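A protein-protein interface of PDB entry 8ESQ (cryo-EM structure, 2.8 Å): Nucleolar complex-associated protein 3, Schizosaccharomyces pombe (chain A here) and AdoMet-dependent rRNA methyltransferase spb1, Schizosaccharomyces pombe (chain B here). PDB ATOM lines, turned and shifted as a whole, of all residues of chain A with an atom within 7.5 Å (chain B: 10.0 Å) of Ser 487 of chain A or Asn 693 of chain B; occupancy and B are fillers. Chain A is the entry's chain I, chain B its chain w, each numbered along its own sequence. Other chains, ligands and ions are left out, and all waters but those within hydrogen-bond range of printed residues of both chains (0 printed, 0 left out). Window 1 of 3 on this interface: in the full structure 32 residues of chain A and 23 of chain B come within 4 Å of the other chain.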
ATOM      1  N   LEU A 394      -1.020 -14.342 -10.587  1.00  0.00           N
ATOM      2  CA  LEU A 394      -1.524 -15.605 -10.057  1.00  0.00           C
ATOM      3  C   LEU A 394      -2.633 -15.370  -9.041  1.00  0.00           C
ATOM      4  O   LEU A 394      -3.620 -16.115  -9.004  1.00  0.00           O
ATOM      5  CB  LEU A 394      -0.383 -16.403  -9.427  1.00  0.00           C
ATOM      6  CG  LEU A 394      -0.771 -17.779  -8.883  1.00  0.00           C
ATOM      7  CD1 LEU A 394      -1.404 -18.621  -9.976  1.00  0.00           C
ATOM      8  CD2 LEU A 394       0.428 -18.487  -8.282  1.00  0.00           C
ATOM      9  N   ILE A 424       3.074 -13.014 -18.582  1.00  0.00           N
ATOM     10  CA  ILE A 424       3.911 -14.185 -18.333  1.00  0.00           C
ATOM     11  C   ILE A 424       3.717 -15.217 -19.436  1.00  0.00           C
ATOM     12  O   ILE A 424       4.681 -15.814 -19.932  1.00  0.00           O
ATOM     13  CB  ILE A 424       3.605 -14.775 -16.944  1.00  0.00           C
ATOM     14  CG1 ILE A 424       3.789 -13.709 -15.863  1.00  0.00           C
ATOM     15  CG2 ILE A 424       4.493 -15.976 -16.667  1.00  0.00           C
ATOM     16  CD1 ILE A 424       2.497 -13.069 -15.409  1.00  0.00           C
ATOM     17  N   LEU A 425       2.465 -15.440 -19.837  1.00  0.00           N
ATOM     18  CA  LEU A 425       2.192 -16.380 -20.917  1.00  0.00           C
ATOM     19  C   LEU A 425       2.574 -15.794 -22.270  1.00  0.00           C
ATOM     20  O   LEU A 425       3.082 -16.509 -23.142  1.00  0.00           O
ATOM     21  CB  LEU A 425       0.717 -16.776 -20.899  1.00  0.00           C
ATOM     22  CG  LEU A 425       0.137 -17.102 -19.523  1.00  0.00           C
ATOM     23  CD1 LEU A 425      -1.352 -17.390 -19.618  1.00  0.00           C
ATOM     24  CD2 LEU A 425       0.875 -18.270 -18.891  1.00  0.00           C
ATOM     25  N   GLN A 480      13.137 -19.336 -12.254  1.00  0.00           N
ATOM     26  CA  GLN A 480      12.432 -20.524 -11.780  1.00  0.00           C
ATOM     27  C   GLN A 480      11.039 -20.178 -11.266  1.00  0.00           C
ATOM     28  O   GLN A 480      10.069 -20.888 -11.560  1.00  0.00           O
ATOM     29  CB  GLN A 480      13.250 -21.216 -10.691  1.00  0.00           C
ATOM     30  CG  GLN A 480      14.540 -21.840 -11.192  1.00  0.00           C
ATOM     31  CD  GLN A 480      15.419 -22.342 -10.063  1.00  0.00           C
ATOM     32  OE1 GLN A 480      15.061 -22.244  -8.890  1.00  0.00           O
ATOM     33  NE2 GLN A 480      16.580 -22.884 -10.415  1.00  0.00           N
ATOM     34  N   ASP A 481      10.919 -19.097 -10.493  1.00  0.00           N
ATOM     35  CA  ASP A 481       9.619 -18.724  -9.941  1.00  0.00           C
ATOM     36  C   ASP A 481       8.644 -18.320 -11.039  1.00  0.00           C
ATOM     37  O   ASP A 481       7.460 -18.669 -10.983  1.00  0.00           O
ATOM     38  CB  ASP A 481       9.782 -17.594  -8.925  1.00  0.00           C
ATOM     39  CG  ASP A 481      10.322 -18.081  -7.596  1.00  0.00           C
ATOM     40  OD1 ASP A 481      10.714 -19.263  -7.511  1.00  0.00           O
ATOM     41  OD2 ASP A 481      10.356 -17.282  -6.636  1.00  0.00           O
ATOM     42  N   LYS A 482       9.121 -17.577 -12.039  1.00  0.00           N
ATOM     43  CA  LYS A 482       8.265 -17.217 -13.164  1.00  0.00           C
ATOM     44  C   LYS A 482       7.820 -18.457 -13.926  1.00  0.00           C
ATOM     45  O   LYS A 482       6.665 -18.549 -14.359  1.00  0.00           O
ATOM     46  CB  LYS A 482       8.997 -16.245 -14.088  1.00  0.00           C
ATOM     47  CG  LYS A 482       8.209 -15.839 -15.320  1.00  0.00           C
ATOM     48  CD  LYS A 482       9.030 -14.931 -16.221  1.00  0.00           C
ATOM     49  CE  LYS A 482       8.294 -14.622 -17.514  1.00  0.00           C
ATOM     50  NZ  LYS A 482       9.133 -13.830 -18.454  1.00  0.00           N
ATOM     51  N   GLU A 483       8.727 -19.419 -14.104  1.00  0.00           N
ATOM     52  CA  GLU A 483       8.371 -20.667 -14.771  1.00  0.00           C
ATOM     53  C   GLU A 483       7.311 -21.426 -13.982  1.00  0.00           C
ATOM     54  O   GLU A 483       6.339 -21.933 -14.554  1.00  0.00           O
ATOM     55  CB  GLU A 483       9.621 -21.525 -14.962  1.00  0.00           C
ATOM     56  CG  GLU A 483       9.498 -22.590 -16.035  1.00  0.00           C
ATOM     57  CD  GLU A 483      10.847 -23.149 -16.444  1.00  0.00           C
ATOM     58  OE1 GLU A 483      11.873 -22.667 -15.923  1.00  0.00           O
ATOM     59  OE2 GLU A 483      10.882 -24.073 -17.283  1.00  0.00           O
ATOM     60  N   LYS A 484       7.484 -21.515 -12.661  1.00  0.00           N
ATOM     61  CA  LYS A 484       6.494 -22.193 -11.831  1.00  0.00           C
ATOM     62  C   LYS A 484       5.169 -21.441 -11.820  1.00  0.00           C
ATOM     63  O   LYS A 484       4.100 -22.057 -11.885  1.00  0.00           O
ATOM     64  CB  LYS A 484       7.028 -22.363 -10.410  1.00  0.00           C
ATOM     65  CG  LYS A 484       6.054 -23.038  -9.459  1.00  0.00           C
ATOM     66  CD  LYS A 484       6.707 -23.333  -8.122  1.00  0.00           C
ATOM     67  CE  LYS A 484       7.057 -22.049  -7.390  1.00  0.00           C
ATOM     68  NZ  LYS A 484       5.842 -21.284  -7.000  1.00  0.00           N
ATOM     69  N   TYR A 485       5.220 -20.110 -11.732  1.00  0.00           N
ATOM     70  CA  TYR A 485       3.991 -19.323 -11.771  1.00  0.00           C
ATOM     71  C   TYR A 485       3.276 -19.489 -13.104  1.00  0.00           C
ATOM     72  O   TYR A 485       2.043 -19.565 -13.151  1.00  0.00           O
ATOM     73  CB  TYR A 485       4.298 -17.849 -11.510  1.00  0.00           C
ATOM     74  CG  TYR A 485       4.483 -17.513 -10.050  1.00  0.00           C
ATOM     75  CD1 TYR A 485       3.857 -18.262  -9.065  1.00  0.00           C
ATOM     76  CD2 TYR A 485       5.272 -16.442  -9.657  1.00  0.00           C
ATOM     77  CE1 TYR A 485       4.016 -17.959  -7.730  1.00  0.00           C
ATOM     78  CE2 TYR A 485       5.437 -16.131  -8.323  1.00  0.00           C
ATOM     79  CZ  TYR A 485       4.807 -16.893  -7.363  1.00  0.00           C
ATOM     80  OH  TYR A 485       4.967 -16.589  -6.031  1.00  0.00           O
ATOM     81  N   GLN A 486       4.035 -19.544 -14.200  1.00  0.00           N
ATOM     82  CA  GLN A 486       3.428 -19.757 -15.508  1.00  0.00           C
ATOM     83  C   GLN A 486       2.717 -21.103 -15.569  1.00  0.00           C
ATOM     84  O   GLN A 486       1.627 -21.212 -16.141  1.00  0.00           O
ATOM     85  CB  GLN A 486       4.494 -19.655 -16.598  1.00  0.00           C
ATOM     86  CG  GLN A 486       4.000 -19.983 -17.995  1.00  0.00           C
ATOM     87  CD  GLN A 486       5.121 -20.018 -19.014  1.00  0.00           C
ATOM     88  OE1 GLN A 486       6.137 -19.340 -18.861  1.00  0.00           O
ATOM     89  NE2 GLN A 486       4.944 -20.813 -20.063  1.00  0.00           N
ATOM     90  N   SER A 487       3.321 -22.140 -14.983  1.00  0.00           N
ATOM     91  CA  SER A 487       2.694 -23.459 -14.975  1.00  0.00           C
ATOM     92  C   SER A 487       1.383 -23.444 -14.201  1.00  0.00           C
ATOM     93  O   SER A 487       0.374 -23.998 -14.654  1.00  0.00           O
ATOM     94  CB  SER A 487       3.653 -24.489 -14.380  1.00  0.00           C
ATOM     95  OG  SER A 487       4.000 -24.151 -13.050  1.00  0.00           O
ATOM     96  N   GLU A 488       1.378 -22.813 -13.026  1.00  0.00           N
ATOM     97  CA  GLU A 488       0.162 -22.773 -12.218  1.00  0.00           C
ATOM     98  C   GLU A 488      -0.918 -21.935 -12.887  1.00  0.00           C
ATOM     99  O   GLU A 488      -2.106 -22.263 -12.802  1.00  0.00           O
ATOM    100  CB  GLU A 488       0.475 -22.237 -10.822  1.00  0.00           C
ATOM    101  CG  GLU A 488       1.468 -23.086 -10.041  1.00  0.00           C
ATOM    102  CD  GLU A 488       1.035 -24.536  -9.914  1.00  0.00           C
ATOM    103  OE1 GLU A 488      -0.184 -24.793  -9.812  1.00  0.00           O
ATOM    104  OE2 GLU A 488       1.916 -25.421  -9.921  1.00  0.00           O
ATOM    105  N   ILE A 489      -0.527 -20.845 -13.550  1.00  0.00           N
ATOM    106  CA  ILE A 489      -1.497 -20.022 -14.265  1.00  0.00           C
ATOM    107  C   ILE A 489      -2.126 -20.813 -15.404  1.00  0.00           C
ATOM    108  O   ILE A 489      -3.343 -20.756 -15.621  1.00  0.00           O
ATOM    109  CB  ILE A 489      -0.831 -18.726 -14.763  1.00  0.00           C
ATOM    110  CG1 ILE A 489      -0.561 -17.788 -13.586  1.00  0.00           C
ATOM    111  CG2 ILE A 489      -1.702 -18.036 -15.792  1.00  0.00           C
ATOM    112  CD1 ILE A 489       0.220 -16.552 -13.960  1.00  0.00           C
ATOM    113  N   LEU A 490      -1.312 -21.569 -16.145  1.00  0.00           N
ATOM    114  CA  LEU A 490      -1.854 -22.431 -17.191  1.00  0.00           C
ATOM    115  C   LEU A 490      -2.802 -23.471 -16.610  1.00  0.00           C
ATOM    116  O   LEU A 490      -3.829 -23.793 -17.218  1.00  0.00           O
ATOM    117  CB  LEU A 490      -0.720 -23.112 -17.956  1.00  0.00           C
ATOM    118  CG  LEU A 490       0.145 -22.219 -18.843  1.00  0.00           C
ATOM    119  CD1 LEU A 490       1.122 -23.055 -19.647  1.00  0.00           C
ATOM    120  CD2 LEU A 490      -0.734 -21.394 -19.765  1.00  0.00           C
ATOM    121  N   LYS A 491      -2.469 -24.012 -15.438  1.00  0.00           N
ATOM    122  CA  LYS A 491      -3.333 -24.998 -14.797  1.00  0.00           C
ATOM    123  C   LYS A 491      -4.704 -24.410 -14.485  1.00  0.00           C
ATOM    124  O   LYS A 491      -5.737 -25.023 -14.777  1.00  0.00           O
ATOM    125  CB  LYS A 491      -2.668 -25.516 -13.522  1.00  0.00           C
ATOM    126  CG  LYS A 491      -3.298 -26.768 -12.946  1.00  0.00           C
ATOM    127  CD  LYS A 491      -2.389 -27.394 -11.902  1.00  0.00           C
ATOM    128  CE  LYS A 491      -2.881 -28.768 -11.488  1.00  0.00           C
ATOM    129  NZ  LYS A 491      -1.893 -29.467 -10.622  1.00  0.00           N
ATOM    130  N   ILE A 492      -4.730 -23.219 -13.886  1.00  0.00           N
ATOM    131  CA  ILE A 492      -5.998 -22.603 -13.503  1.00  0.00           C
ATOM    132  C   ILE A 492      -6.765 -22.144 -14.737  1.00  0.00           C
ATOM    133  O   ILE A 492      -7.986 -22.313 -14.830  1.00  0.00           O
ATOM    134  CB  ILE A 492      -5.750 -21.442 -12.526  1.00  0.00           C
ATOM    135  CG1 ILE A 492      -4.932 -21.931 -11.332  1.00  0.00           C
ATOM    136  CG2 ILE A 492      -7.063 -20.857 -12.056  1.00  0.00           C
ATOM    137  CD1 ILE A 492      -4.236 -20.829 -10.583  1.00  0.00           C
ATOM    138  N   ILE A 493      -6.062 -21.541 -15.697  1.00  0.00           N
ATOM    139  CA  ILE A 493      -6.729 -21.010 -16.881  1.00  0.00           C
ATOM    140  C   ILE A 493      -7.328 -22.136 -17.714  1.00  0.00           C
ATOM    141  O   ILE A 493      -8.492 -22.069 -18.128  1.00  0.00           O
ATOM    142  CB  ILE A 493      -5.751 -20.154 -17.705  1.00  0.00           C
ATOM    143  CG1 ILE A 493      -5.558 -18.788 -17.048  1.00  0.00           C
ATOM    144  CG2 ILE A 493      -6.249 -19.993 -19.124  1.00  0.00           C
ATOM    145  CD1 ILE A 493      -4.667 -17.858 -17.837  1.00  0.00           C
ATOM    146  N   HIS A 520       0.236 -23.335 -27.578  1.00  0.00           N
ATOM    147  CA  HIS A 520       1.670 -23.529 -27.768  1.00  0.00           C
ATOM    148  C   HIS A 520       2.434 -23.538 -26.451  1.00  0.00           C
ATOM    149  O   HIS A 520       3.569 -24.024 -26.408  1.00  0.00           O
ATOM    150  CB  HIS A 520       2.227 -22.446 -28.696  1.00  0.00           C
ATOM    151  CG  HIS A 520       2.098 -21.057 -28.155  1.00  0.00           C
ATOM    152  ND1 HIS A 520       3.190 -20.276 -27.841  1.00  0.00           N
ATOM    153  CD2 HIS A 520       1.007 -20.306 -27.880  1.00  0.00           C
ATOM    154  CE1 HIS A 520       2.775 -19.104 -27.391  1.00  0.00           C
ATOM    155  NE2 HIS A 520       1.454 -19.097 -27.405  1.00  0.00           N
ATOM    156  N   LEU A 521       1.839 -23.014 -25.378  1.00  0.00           N
ATOM    157  CA  LEU A 521       2.473 -23.026 -24.066  1.00  0.00           C
ATOM    158  C   LEU A 521       2.379 -24.379 -23.373  1.00  0.00           C
ATOM    159  O   LEU A 521       3.161 -24.643 -22.454  1.00  0.00           O
ATOM    160  CB  LEU A 521       1.839 -21.956 -23.176  1.00  0.00           C
ATOM    161  CG  LEU A 521       2.012 -20.503 -23.614  1.00  0.00           C
ATOM    162  CD1 LEU A 521       0.870 -19.659 -23.093  1.00  0.00           C
ATOM    163  CD2 LEU A 521       3.332 -19.966 -23.101  1.00  0.00           C
ATOM    164  N   LEU A 522       1.450 -25.235 -23.788  1.00  0.00           N
ATOM    165  CA  LEU A 522       1.183 -26.477 -23.084  1.00  0.00           C
ATOM    166  C   LEU A 522       2.108 -27.592 -23.569  1.00  0.00           C
ATOM    167  O   LEU A 522       2.835 -27.454 -24.556  1.00  0.00           O
ATOM    168  CB  LEU A 522      -0.280 -26.878 -23.261  1.00  0.00           C
ATOM    169  CG  LEU A 522      -0.948 -27.488 -22.033  1.00  0.00           C
ATOM    170  CD1 LEU A 522      -0.833 -26.539 -20.855  1.00  0.00           C
ATOM    171  CD2 LEU A 522      -2.403 -27.808 -22.322  1.00  0.00           C
ATOM    172  N   ASN A 523       2.063 -28.719 -22.860  1.00  0.00           N
ATOM    173  CA  ASN A 523       2.921 -29.852 -23.173  1.00  0.00           C
ATOM    174  C   ASN A 523       2.520 -30.496 -24.498  1.00  0.00           C
ATOM    175  O   ASN A 523       1.398 -30.338 -24.988  1.00  0.00           O
ATOM    176  CB  ASN A 523       2.870 -30.896 -22.057  1.00  0.00           C
ATOM    177  CG  ASN A 523       3.617 -30.459 -20.814  1.00  0.00           C
ATOM    178  OD1 ASN A 523       4.643 -29.785 -20.896  1.00  0.00           O
ATOM    179  ND2 ASN A 523       3.105 -30.843 -19.651  1.00  0.00           N
ATOM    180  N   PHE A 526      -0.402 -33.010 -24.425  1.00  0.00           N
ATOM    181  CA  PHE A 526      -1.716 -32.386 -24.382  1.00  0.00           C
ATOM    182  C   PHE A 526      -2.167 -31.891 -25.750  1.00  0.00           C
ATOM    183  O   PHE A 526      -3.374 -31.789 -25.988  1.00  0.00           O
ATOM    184  CB  PHE A 526      -1.713 -31.237 -23.376  1.00  0.00           C
ATOM    185  CG  PHE A 526      -1.680 -31.693 -21.946  1.00  0.00           C
ATOM    186  CD1 PHE A 526      -2.118 -32.961 -21.603  1.00  0.00           C
ATOM    187  CD2 PHE A 526      -1.198 -30.864 -20.949  1.00  0.00           C
ATOM    188  CE1 PHE A 526      -2.086 -33.388 -20.292  1.00  0.00           C
ATOM    189  CE2 PHE A 526      -1.162 -31.287 -19.636  1.00  0.00           C
ATOM    190  CZ  PHE A 526      -1.608 -32.550 -19.306  1.00  0.00           C
ATOM    191  N   LYS B 688       3.054 -36.441 -11.210  1.00  0.00           N
ATOM    192  CA  LYS B 688       2.488 -35.309 -10.482  1.00  0.00           C
ATOM    193  C   LYS B 688       3.342 -34.060 -10.647  1.00  0.00           C
ATOM    194  O   LYS B 688       2.817 -32.964 -10.880  1.00  0.00           O
ATOM    195  CB  LYS B 688       2.339 -35.649  -9.000  1.00  0.00           C
ATOM    196  CG  LYS B 688       1.287 -36.689  -8.675  1.00  0.00           C
ATOM    197  CD  LYS B 688       0.756 -36.469  -7.264  1.00  0.00           C
ATOM    198  CE  LYS B 688      -0.669 -36.965  -7.108  1.00  0.00           C
ATOM    199  NZ  LYS B 688      -1.216 -36.669  -5.756  1.00  0.00           N
ATOM    200  N   MET B 689       4.663 -34.202 -10.528  1.00  0.00           N
ATOM    201  CA  MET B 689       5.550 -33.049 -10.618  1.00  0.00           C
ATOM    202  C   MET B 689       5.672 -32.519 -12.039  1.00  0.00           C
ATOM    203  O   MET B 689       6.233 -31.435 -12.235  1.00  0.00           O
ATOM    204  CB  MET B 689       6.932 -33.403 -10.069  1.00  0.00           C
ATOM    205  CG  MET B 689       7.041 -33.330  -8.551  1.00  0.00           C
ATOM    206  SD  MET B 689       5.657 -34.102  -7.688  1.00  0.00           S
ATOM    207  CE  MET B 689       4.903 -32.684  -6.896  1.00  0.00           C
ATOM    208  N   LYS B 690       5.174 -33.254 -13.033  1.00  0.00           N
ATOM    209  CA  LYS B 690       5.206 -32.778 -14.409  1.00  0.00           C
ATOM    210  C   LYS B 690       4.264 -31.597 -14.587  1.00  0.00           C
ATOM    211  O   LYS B 690       3.040 -31.767 -14.615  1.00  0.00           O
ATOM    212  CB  LYS B 690       4.839 -33.903 -15.377  1.00  0.00           C
ATOM    213  CG  LYS B 690       4.813 -33.471 -16.834  1.00  0.00           C
ATOM    214  CD  LYS B 690       4.486 -34.634 -17.752  1.00  0.00           C
ATOM    215  CE  LYS B 690       5.669 -35.576 -17.888  1.00  0.00           C
ATOM    216  NZ  LYS B 690       6.808 -34.932 -18.597  1.00  0.00           N
ATOM    217  N   ALA B 691       4.824 -30.397 -14.705  1.00  0.00           N
ATOM    218  CA  ALA B 691       4.014 -29.201 -14.864  1.00  0.00           C
ATOM    219  C   ALA B 691       3.397 -29.148 -16.259  1.00  0.00           C
ATOM    220  O   ALA B 691       3.850 -29.808 -17.197  1.00  0.00           O
ATOM    221  CB  ALA B 691       4.852 -27.949 -14.611  1.00  0.00           C
ATOM    222  N   LEU B 692       2.339 -28.343 -16.381  1.00  0.00           N
ATOM    223  CA  LEU B 692       1.658 -28.203 -17.664  1.00  0.00           C
ATOM    224  C   LEU B 692       2.573 -27.619 -18.731  1.00  0.00           C
ATOM    225  O   LEU B 692       2.404 -27.911 -19.920  1.00  0.00           O
ATOM    226  CB  LEU B 692       0.412 -27.333 -17.507  1.00  0.00           C
ATOM    227  CG  LEU B 692      -0.848 -28.014 -16.974  1.00  0.00           C
ATOM    228  CD1 LEU B 692      -0.768 -28.228 -15.472  1.00  0.00           C
ATOM    229  CD2 LEU B 692      -2.070 -27.196 -17.339  1.00  0.00           C
ATOM    230  N   ASN B 693       3.536 -26.787 -18.335  1.00  0.00           N
ATOM    231  CA  ASN B 693       4.487 -26.196 -19.266  1.00  0.00           C
ATOM    232  C   ASN B 693       5.878 -26.804 -19.129  1.00  0.00           C
ATOM    233  O   ASN B 693       6.872 -26.152 -19.462  1.00  0.00           O
ATOM    234  CB  ASN B 693       4.548 -24.681 -19.075  1.00  0.00           C
ATOM    235  CG  ASN B 693       5.018 -24.281 -17.689  1.00  0.00           C
ATOM    236  OD1 ASN B 693       5.395 -25.125 -16.876  1.00  0.00           O
ATOM    237  ND2 ASN B 693       5.001 -22.984 -17.414  1.00  0.00           N
ATOM    238  N   ALA B 694       5.968 -28.031 -18.612  1.00  0.00           N
ATOM    239  CA  ALA B 694       7.271 -28.668 -18.454  1.00  0.00           C
ATOM    240  C   ALA B 694       7.935 -28.911 -19.802  1.00  0.00           C
ATOM    241  O   ALA B 694       9.145 -28.705 -19.953  1.00  0.00           O
ATOM    242  CB  ALA B 694       7.124 -29.979 -17.682  1.00  0.00           C
ATOM    243  N   ARG B 695       7.164 -29.354 -20.792  1.00  0.00           N
ATOM    244  CA  ARG B 695       7.685 -29.677 -22.120  1.00  0.00           C
ATOM    245  C   ARG B 695       6.779 -29.100 -23.203  1.00  0.00           C
ATOM    246  O   ARG B 695       6.095 -29.839 -23.919  1.00  0.00           O
ATOM    247  CB  ARG B 695       7.838 -31.190 -22.273  1.00  0.00           C
ATOM    248  CG  ARG B 695       8.816 -31.615 -23.344  1.00  0.00           C
ATOM    249  CD  ARG B 695       8.908 -33.126 -23.411  1.00  0.00           C
ATOM    250  NE  ARG B 695       7.724 -33.736 -24.000  1.00  0.00           N
ATOM    251  CZ  ARG B 695       7.528 -35.044 -24.094  1.00  0.00           C
ATOM    252  NH1 ARG B 695       8.424 -35.909 -23.649  1.00  0.00           N
ATOM    253  NH2 ARG B 695       6.406 -35.494 -24.646  1.00  0.00           N
ATOM    254  N   PRO B 696       6.754 -27.768 -23.355  1.00  0.00           N
ATOM    255  CA  PRO B 696       6.004 -27.168 -24.466  1.00  0.00           C
ATOM    256  C   PRO B 696       6.709 -27.338 -25.801  1.00  0.00           C
ATOM    257  O   PRO B 696       7.725 -28.034 -25.889  1.00  0.00           O
ATOM    258  CB  PRO B 696       5.906 -25.692 -24.063  1.00  0.00           C
ATOM    259  CG  PRO B 696       7.108 -25.462 -23.234  1.00  0.00           C
ATOM    260  CD  PRO B 696       7.335 -26.740 -22.475  1.00  0.00           C
ATOM    261  N   ILE B 697       6.169 -26.706 -26.846  1.00  0.00           N
ATOM    262  CA  ILE B 697       6.691 -26.906 -28.196  1.00  0.00           C
ATOM    263  C   ILE B 697       8.140 -26.440 -28.288  1.00  0.00           C
ATOM    264  O   ILE B 697       8.982 -27.101 -28.908  1.00  0.00           O
ATOM    265  CB  ILE B 697       5.800 -26.199 -29.234  1.00  0.00           C
ATOM    266  CG1 ILE B 697       5.658 -24.709 -28.917  1.00  0.00           C
ATOM    267  CG2 ILE B 697       4.427 -26.847 -29.282  1.00  0.00           C
ATOM    268  CD1 ILE B 697       5.192 -23.884 -30.092  1.00  0.00           C
ATOM    269  N   LYS B 698       8.456 -25.296 -27.678  1.00  0.00           N
ATOM    270  CA  LYS B 698       9.833 -24.814 -27.714  1.00  0.00           C
ATOM    271  C   LYS B 698      10.749 -25.701 -26.878  1.00  0.00           C
ATOM    272  O   LYS B 698      11.806 -26.134 -27.348  1.00  0.00           O
ATOM    273  CB  LYS B 698       9.904 -23.357 -27.250  1.00  0.00           C
ATOM    274  CG  LYS B 698       9.361 -23.094 -25.857  1.00  0.00           C
ATOM    275  CD  LYS B 698       9.473 -21.626 -25.515  1.00  0.00           C
ATOM    276  CE  LYS B 698      10.926 -21.185 -25.528  1.00  0.00           C
ATOM    277  NZ  LYS B 698      11.055 -19.733 -25.821  1.00  0.00           N
ATOM    278  N   LYS B 699      10.341 -26.024 -25.649  1.00  0.00           N
ATOM    279  CA  LYS B 699      11.220 -26.782 -24.765  1.00  0.00           C
ATOM    280  C   LYS B 699      11.403 -28.219 -25.230  1.00  0.00           C
ATOM    281  O   LYS B 699      12.212 -28.948 -24.647  1.00  0.00           O
ATOM    282  CB  LYS B 699      10.689 -26.758 -23.333  1.00  0.00           C
ATOM    283  CG  LYS B 699      10.840 -25.414 -22.645  1.00  0.00           C
ATOM    284  CD  LYS B 699      10.363 -25.474 -21.207  1.00  0.00           C
ATOM    285  CE  LYS B 699      10.383 -24.100 -20.566  1.00  0.00           C
ATOM    286  NZ  LYS B 699       9.733 -24.114 -19.229  1.00  0.00           N
ATOM    287  N   VAL B 700      10.654 -28.651 -26.241  1.00  0.00           N
ATOM    288  CA  VAL B 700      10.862 -29.970 -26.825  1.00  0.00           C
ATOM    289  C   VAL B 700      11.561 -29.901 -28.181  1.00  0.00           C
ATOM    290  O   VAL B 700      12.165 -30.900 -28.602  1.00  0.00           O
ATOM    291  CB  VAL B 700       9.526 -30.730 -26.954  1.00  0.00           C
ATOM    292  CG1 VAL B 700       8.729 -30.199 -28.130  1.00  0.00           C
ATOM    293  CG2 VAL B 700       9.765 -32.227 -27.085  1.00  0.00           C
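Ser 487 of chain A touches just these residues of chain B: Ala 691 (3.7 Å) and Asn 693 (3.1 Å). Asn 693 of chain B touches just these residues of chain A: Glu 483 (3.3 Å), Gln 486 (3.2 Å), Ser 487 (3.1 Å), Leu 490 (3.8 Å), Leu 521 (3.7 Å) and Asn 523 (3.7 Å). Leu 490 of chain A touches just these residues of chain B: Leu 692 (3.8 Å) and Asn 693 (3.8 Å). Of the printed residues of chain A, Arg 695 of chain B touches Asn 523 (2.6 Å). Of the printed residues of chain B, His 520 of chain A touches Pro 696 (3.7 Å) and Ile 697 (3.3 Å). Printed residues of chain B within 4 Å of Leu 521 of chain A: Asn 693 (3.7 Å) and Pro 696 (3.4 Å). Of the printed residues of chain A, Lys 699 of chain B touches Glu 483 (2.3 Å). Printed residues of chain A within 4 Å of Ile 697 of chain B: His 520. Asp 481 of chain A touches none of the printed residues of chain B. The nearest residue of chain B that does not touch Ser 487 of chain A is Leu 692 of chain B (4.4 Å). The nearest printed residue of chain A that does not touch Lys 699 of chain B is Gln 486 of chain A (5.9 Å).
O of Glu 483 of chain A is in hydrogen-bond range of ND2 of Asn 693 of chain B, at 3.3 Å. The side-chain amide nitrogen (ND2) of Asn 693 of chain B lies close to the side-chain amide nitrogen (NE2) of Gln 486 of chain A, at 3.4 Å. ND2 of Asn 693 of chain B lies close to N of Ser 487 of chain A, 3.1 Å away. The backbone carbonyl oxygen (O) of Ala 691 of chain B lies within hydrogen-bond range of the side-chain amide nitrogen (ND2) of Asn 523 of chain A, at 2.8 Å. ND2 of Asn 523 of chain A lies close to O of Leu 692 of chain B (3.0 Å). N of Ala 694 of chain B lies within hydrogen-bond range of OD1 of Asn 523 of chain A (3.2 Å). The backbone NH (N) of Arg 695 of chain B sits at hydrogen-bond distance from the side-chain amide oxygen (OD1) of Asn 523 of chain A (2.6 Å). The side-chain carboxylate (OE2) of Glu 483 of chain A lies close to the side-chain amino group (NZ) of Lys 699 of chain B (2.3 Å).
Of the 13 printed residues of chain B, 8 touch a printed residue of chain A. Hydrophobic or aromatic side chains of chain B within 4 Å of the printed part of chain A: Ala 691, Leu 692, Pro 696 and Ile 697. Hydrophobic or aromatic side chains of chain A that line the printed part of chain B: Leu 490, His 520 and Leu 522. Among the printed residues, 20 pairs touch across the chains. Among the printed residues, Asp or Glu carboxylates within 4 Å of a Lys or Arg side-chain nitrogen of the other chain: Glu 483 of chain A with Lys 699 of chain B.
Among the printed residues, pairs that only touch across the chains: Leu 522 of chain A with Pro 696 of chain B (3.2 Å), His 520 of chain A with Ile 697 of chain B (3.3 Å), Leu 521 of chain A with Pro 696 of chain B (3.4 Å), Lys 491 of chain A with Leu 692 of chain B (3.6 Å), Leu 522 of chain A with Leu 692 of chain B (3.6 Å), Leu 521 of chain A with Asn 693 of chain B (3.7 Å), Ser 487 of chain A with Ala 691 of chain B (3.7 Å), Asn 523 of chain A with Asn 693 of chain B (3.7 Å), His 520 of chain A with Pro 696 of chain B (3.7 Å), Asn 523 of chain A with Pro 696 of chain B (3.8 Å), Leu 490 of chain A with Leu 692 of chain B (3.8 Å) and Leu 490 of chain A with Asn 693 of chain B (3.8 Å).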
